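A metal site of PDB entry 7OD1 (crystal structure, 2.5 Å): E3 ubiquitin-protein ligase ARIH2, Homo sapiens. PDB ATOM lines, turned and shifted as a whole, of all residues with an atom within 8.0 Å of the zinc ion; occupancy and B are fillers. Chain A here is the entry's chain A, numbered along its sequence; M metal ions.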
ATOM      1  N   CYS A  63       7.032 -27.355  21.939  1.00  0.00           N
ATOM      2  CA  CYS A  63       8.182 -26.486  22.188  1.00  0.00           C
ATOM      3  C   CYS A  63       9.430 -27.156  21.629  1.00  0.00           C
ATOM      4  O   CYS A  63       9.872 -28.194  22.130  1.00  0.00           O
ATOM      5  CB  CYS A  63       8.348 -26.204  23.686  1.00  0.00           C
ATOM      6  SG  CYS A  63       7.037 -25.184  24.410  1.00  0.00           S
ATOM      7  N   LEU A 227       8.436 -17.775  16.807  1.00  0.00           N
ATOM      8  CA  LEU A 227       9.529 -17.579  17.745  1.00  0.00           C
ATOM      9  C   LEU A 227       8.982 -17.226  19.125  1.00  0.00           C
ATOM     10  O   LEU A 227       7.987 -16.499  19.239  1.00  0.00           O
ATOM     11  CB  LEU A 227      10.477 -16.481  17.255  1.00  0.00           C
ATOM     12  CG  LEU A 227      11.375 -16.823  16.065  1.00  0.00           C
ATOM     13  CD1 LEU A 227      12.084 -15.578  15.580  1.00  0.00           C
ATOM     14  CD2 LEU A 227      12.372 -17.905  16.443  1.00  0.00           C
ATOM     15  N   CYS A 228       9.626 -17.741  20.153  1.00  0.00           N
ATOM     16  CA  CYS A 228       9.211 -17.442  21.515  1.00  0.00           C
ATOM     17  C   CYS A 228       9.491 -15.977  21.813  1.00  0.00           C
ATOM     18  O   CYS A 228      10.634 -15.535  21.664  1.00  0.00           O
ATOM     19  CB  CYS A 228       9.933 -18.340  22.502  1.00  0.00           C
ATOM     20  SG  CYS A 228       9.504 -18.036  24.230  1.00  0.00           S
ATOM     21  N   PRO A 229       8.496 -15.193  22.245  1.00  0.00           N
ATOM     22  CA  PRO A 229       8.758 -13.775  22.537  1.00  0.00           C
ATOM     23  C   PRO A 229       9.590 -13.545  23.783  1.00  0.00           C
ATOM     24  O   PRO A 229       9.943 -12.392  24.051  1.00  0.00           O
ATOM     25  CB  PRO A 229       7.343 -13.180  22.702  1.00  0.00           C
ATOM     26  CG  PRO A 229       6.373 -14.284  22.348  1.00  0.00           C
ATOM     27  CD  PRO A 229       7.094 -15.571  22.503  1.00  0.00           C
ATOM     28  N   GLY A 230       9.905 -14.589  24.539  1.00  0.00           N
ATOM     29  CA  GLY A 230      10.699 -14.417  25.739  1.00  0.00           C
ATOM     30  C   GLY A 230      12.067 -13.827  25.431  1.00  0.00           C
ATOM     31  O   GLY A 230      12.675 -14.108  24.390  1.00  0.00           O
ATOM     32  N   ALA A 231      12.552 -13.010  26.366  1.00  0.00           N
ATOM     33  CA  ALA A 231      13.827 -12.334  26.181  1.00  0.00           C
ATOM     34  C   ALA A 231      14.968 -13.347  26.108  1.00  0.00           C
ATOM     35  O   ALA A 231      15.180 -14.117  27.044  1.00  0.00           O
ATOM     36  CB  ALA A 231      14.062 -11.356  27.327  1.00  0.00           C
ATOM     37  N   ASP A 232      15.682 -13.344  24.978  1.00  0.00           N
ATOM     38  CA  ASP A 232      16.837 -14.208  24.763  1.00  0.00           C
ATOM     39  C   ASP A 232      16.469 -15.683  24.900  1.00  0.00           C
ATOM     40  O   ASP A 232      17.245 -16.494  25.418  1.00  0.00           O
ATOM     41  CB  ASP A 232      17.991 -13.849  25.707  1.00  0.00           C
ATOM     42  CG  ASP A 232      18.358 -12.374  25.645  1.00  0.00           C
ATOM     43  OD1 ASP A 232      17.985 -11.706  24.655  1.00  0.00           O
ATOM     44  OD2 ASP A 232      19.002 -11.882  26.590  1.00  0.00           O
ATOM     45  N   CYS A 233      15.268 -16.047  24.446  1.00  0.00           N
ATOM     46  CA  CYS A 233      14.799 -17.420  24.553  1.00  0.00           C
ATOM     47  C   CYS A 233      14.985 -18.123  23.216  1.00  0.00           C
ATOM     48  O   CYS A 233      14.340 -17.725  22.229  1.00  0.00           O
ATOM     49  CB  CYS A 233      13.339 -17.456  24.979  1.00  0.00           C
ATOM     50  SG  CYS A 233      12.750 -19.126  25.301  1.00  0.00           S
ATOM     51  N   PRO A 234      15.813 -19.159  23.143  1.00  0.00           N
ATOM     52  CA  PRO A 234      16.047 -19.884  21.878  1.00  0.00           C
ATOM     53  C   PRO A 234      15.069 -21.033  21.652  1.00  0.00           C
ATOM     54  O   PRO A 234      15.462 -22.164  21.371  1.00  0.00           O
ATOM     55  CB  PRO A 234      17.475 -20.381  22.031  1.00  0.00           C
ATOM     56  CG  PRO A 234      17.563 -20.687  23.507  1.00  0.00           C
ATOM     57  CD  PRO A 234      16.685 -19.668  24.218  1.00  0.00           C
ATOM     58  N   MET A 235      13.768 -20.750  21.794  1.00  0.00           N
ATOM     59  CA  MET A 235      12.736 -21.755  21.626  1.00  0.00           C
ATOM     60  C   MET A 235      11.756 -21.329  20.539  1.00  0.00           C
ATOM     61  O   MET A 235      11.555 -20.129  20.293  1.00  0.00           O
ATOM     62  CB  MET A 235      11.990 -22.021  22.939  1.00  0.00           C
ATOM     63  CG  MET A 235      12.862 -22.606  24.034  1.00  0.00           C
ATOM     64  SD  MET A 235      13.457 -24.266  23.643  1.00  0.00           S
ATOM     65  CE  MET A 235      11.934 -25.216  23.711  1.00  0.00           C
ATOM     66  N   VAL A 236      11.141 -22.314  19.909  1.00  0.00           N
ATOM     67  CA  VAL A 236      10.146 -22.096  18.859  1.00  0.00           C
ATOM     68  C   VAL A 236       8.898 -22.880  19.245  1.00  0.00           C
ATOM     69  O   VAL A 236       8.984 -24.022  19.710  1.00  0.00           O
ATOM     70  CB  VAL A 236      10.672 -22.541  17.483  1.00  0.00           C
ATOM     71  CG1 VAL A 236       9.569 -22.518  16.439  1.00  0.00           C
ATOM     72  CG2 VAL A 236      11.837 -21.653  17.041  1.00  0.00           C
ATOM     73  N   ILE A 237       7.736 -22.267  19.062  1.00  0.00           N
ATOM     74  CA  ILE A 237       6.464 -22.919  19.351  1.00  0.00           C
ATOM     75  C   ILE A 237       5.885 -23.399  18.016  1.00  0.00           C
ATOM     76  O   ILE A 237       5.729 -22.609  17.086  1.00  0.00           O
ATOM     77  CB  ILE A 237       5.485 -21.982  20.081  1.00  0.00           C
ATOM     78  CG1 ILE A 237       5.780 -21.911  21.587  1.00  0.00           C
ATOM     79  CG2 ILE A 237       4.060 -22.452  19.878  1.00  0.00           C
ATOM     80  CD1 ILE A 237       7.143 -21.379  21.974  1.00  0.00           C
ATOM     81  N   GLN A 248       2.404 -21.570  25.624  1.00  0.00           N
ATOM     82  CA  GLN A 248       3.352 -21.248  26.675  1.00  0.00           C
ATOM     83  C   GLN A 248       4.664 -21.976  26.411  1.00  0.00           C
ATOM     84  O   GLN A 248       4.671 -23.208  26.296  1.00  0.00           O
ATOM     85  CB  GLN A 248       2.798 -21.629  28.050  1.00  0.00           C
ATOM     86  CG  GLN A 248       3.745 -21.312  29.199  1.00  0.00           C
ATOM     87  CD  GLN A 248       3.125 -21.556  30.559  1.00  0.00           C
ATOM     88  OE1 GLN A 248       1.958 -21.934  30.657  1.00  0.00           O
ATOM     89  NE2 GLN A 248       3.901 -21.360  31.609  1.00  0.00           N
ATOM     90  N   CYS A 249       5.752 -21.224  26.328  1.00  0.00           N
ATOM     91  CA  CYS A 249       7.065 -21.830  26.187  1.00  0.00           C
ATOM     92  C   CYS A 249       7.458 -22.542  27.476  1.00  0.00           C
ATOM     93  O   CYS A 249       7.282 -22.006  28.571  1.00  0.00           O
ATOM     94  CB  CYS A 249       8.101 -20.757  25.836  1.00  0.00           C
ATOM     95  SG  CYS A 249       9.818 -21.274  26.005  1.00  0.00           S
ATOM     96  N   ASN A 250       7.989 -23.753  27.343  1.00  0.00           N
ATOM     97  CA  ASN A 250       8.315 -24.563  28.513  1.00  0.00           C
ATOM     98  C   ASN A 250       9.703 -24.301  29.075  1.00  0.00           C
ATOM     99  O   ASN A 250      10.094 -24.967  30.041  1.00  0.00           O
ATOM    100  CB  ASN A 250       8.164 -26.056  28.174  1.00  0.00           C
ATOM    101  CG  ASN A 250       9.086 -26.503  27.057  1.00  0.00           C
ATOM    102  OD1 ASN A 250       9.878 -25.722  26.528  1.00  0.00           O
ATOM    103  ND2 ASN A 250       8.993 -27.784  26.701  1.00  0.00           N
ATOM    104  N   ARG A 251      10.441 -23.345  28.518  1.00  0.00           N
ATOM    105  CA  ARG A 251      11.774 -23.031  29.005  1.00  0.00           C
ATOM    106  C   ARG A 251      11.818 -21.733  29.815  1.00  0.00           C
ATOM    107  O   ARG A 251      12.514 -21.672  30.833  1.00  0.00           O
ATOM    108  CB  ARG A 251      12.760 -22.932  27.836  1.00  0.00           C
ATOM    109  CG  ARG A 251      13.684 -24.139  27.699  1.00  0.00           C
ATOM    110  CD  ARG A 251      12.890 -25.439  27.615  1.00  0.00           C
ATOM    111  NE  ARG A 251      13.732 -26.584  27.257  1.00  0.00           N
ATOM    112  CZ  ARG A 251      13.288 -27.699  26.709  1.00  0.00           C
ATOM    113  NH1 ARG A 251      12.007 -27.863  26.422  1.00  0.00           N
ATOM    114  NH2 ARG A 251      14.146 -28.671  26.425  1.00  0.00           N
ATOM    115  N   CYS A 252      11.075 -20.711  29.386  1.00  0.00           N
ATOM    116  CA  CYS A 252      10.995 -19.459  30.113  1.00  0.00           C
ATOM    117  C   CYS A 252       9.582 -19.125  30.588  1.00  0.00           C
ATOM    118  O   CYS A 252       9.380 -18.062  31.184  1.00  0.00           O
ATOM    119  CB  CYS A 252      11.535 -18.306  29.255  1.00  0.00           C
ATOM    120  SG  CYS A 252      10.423 -17.806  27.924  1.00  0.00           S
ATOM    121  N   ASN A 253       8.613 -19.999  30.325  1.00  0.00           N
ATOM    122  CA  ASN A 253       7.236 -19.878  30.812  1.00  0.00           C
ATOM    123  C   ASN A 253       6.522 -18.647  30.256  1.00  0.00           C
ATOM    124  O   ASN A 253       5.532 -18.190  30.832  1.00  0.00           O
ATOM    125  CB  ASN A 253       7.187 -19.874  32.343  1.00  0.00           C
ATOM    126  CG  ASN A 253       7.591 -21.207  32.935  1.00  0.00           C
ATOM    127  OD1 ASN A 253       6.892 -22.215  32.766  1.00  0.00           O
ATOM    128  ND2 ASN A 253       8.727 -21.234  33.626  1.00  0.00           N
ATOM    129  N   GLU A 254       7.000 -18.105  29.136  1.00  0.00           N
ATOM    130  CA  GLU A 254       6.297 -16.991  28.493  1.00  0.00           C
ATOM    131  C   GLU A 254       5.008 -17.483  27.863  1.00  0.00           C
ATOM    132  O   GLU A 254       5.002 -18.434  27.080  1.00  0.00           O
ATOM    133  CB  GLU A 254       7.195 -16.353  27.431  1.00  0.00           C
ATOM    134  CG  GLU A 254       6.563 -15.164  26.721  1.00  0.00           C
ATOM    135  CD  GLU A 254       6.875 -13.841  27.397  1.00  0.00           C
ATOM    136  OE1 GLU A 254       7.944 -13.740  28.047  1.00  0.00           O
ATOM    137  OE2 GLU A 254       6.056 -12.909  27.281  1.00  0.00           O
ATOM    138  N   VAL A 255       3.899 -16.832  28.212  1.00  0.00           N
ATOM    139  CA  VAL A 255       2.585 -17.141  27.677  1.00  0.00           C
ATOM    140  C   VAL A 255       2.236 -16.107  26.618  1.00  0.00           C
ATOM    141  O   VAL A 255       2.514 -14.918  26.795  1.00  0.00           O
ATOM    142  CB  VAL A 255       1.516 -17.172  28.788  1.00  0.00           C
ATOM    143  CG1 VAL A 255       0.157 -17.548  28.227  1.00  0.00           C
ATOM    144  CG2 VAL A 255       1.923 -18.137  29.896  1.00  0.00           C
ATOM    145  N   PHE A 256       1.619 -16.553  25.521  1.00  0.00           N
ATOM    146  CA  PHE A 256       1.282 -15.621  24.452  1.00  0.00           C
ATOM    147  C   PHE A 256       0.303 -16.273  23.481  1.00  0.00           C
ATOM    148  O   PHE A 256       0.118 -17.492  23.460  1.00  0.00           O
ATOM    149  CB  PHE A 256       2.533 -15.128  23.710  1.00  0.00           C
ATOM    150  CG  PHE A 256       3.335 -16.217  23.049  1.00  0.00           C
ATOM    151  CD1 PHE A 256       4.089 -17.114  23.809  1.00  0.00           C
ATOM    152  CD2 PHE A 256       3.351 -16.340  21.674  1.00  0.00           C
ATOM    153  CE1 PHE A 256       4.822 -18.115  23.203  1.00  0.00           C
ATOM    154  CE2 PHE A 256       4.097 -17.340  21.052  1.00  0.00           C
ATOM    155  CZ  PHE A 256       4.830 -18.221  21.822  1.00  0.00           C
HETATM  156 ZN    ZN M   1      10.552 -19.082  26.004  1.00  0.00          ZN
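SG of Cys 233 binds the zinc ion (2.3 Å). The side-chain sulfur (SG) of Cys 252 is bound to the zinc ion, 2.3 Å away. The zinc ion is bound by SG of Cys 228 (2.3 Å). The zinc ion is bound by the side-chain sulfur (SG) of Cys 249. The zinc ion has four donor atoms within binding distance.
The nearest printed residue that does not touch the zinc ion is Met 235 (4.5 Å).
The backbone NH of Cys 228 sits at hydrogen-bond distance from the backbone carbonyl oxygen of Met 235 (3.1 Å). The backbone NH (N) of Cys 249 is in hydrogen-bond range of the backbone carbonyl oxygen (O) of Glu 254. N of Gly 230 lies close to SG of Cys 228 (3.5 Å). SG of Cys 252 lies close to N of Glu 254 (3.6 Å). SG of Cys 249 lies close to N of Arg 251, 3.3 Å away.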
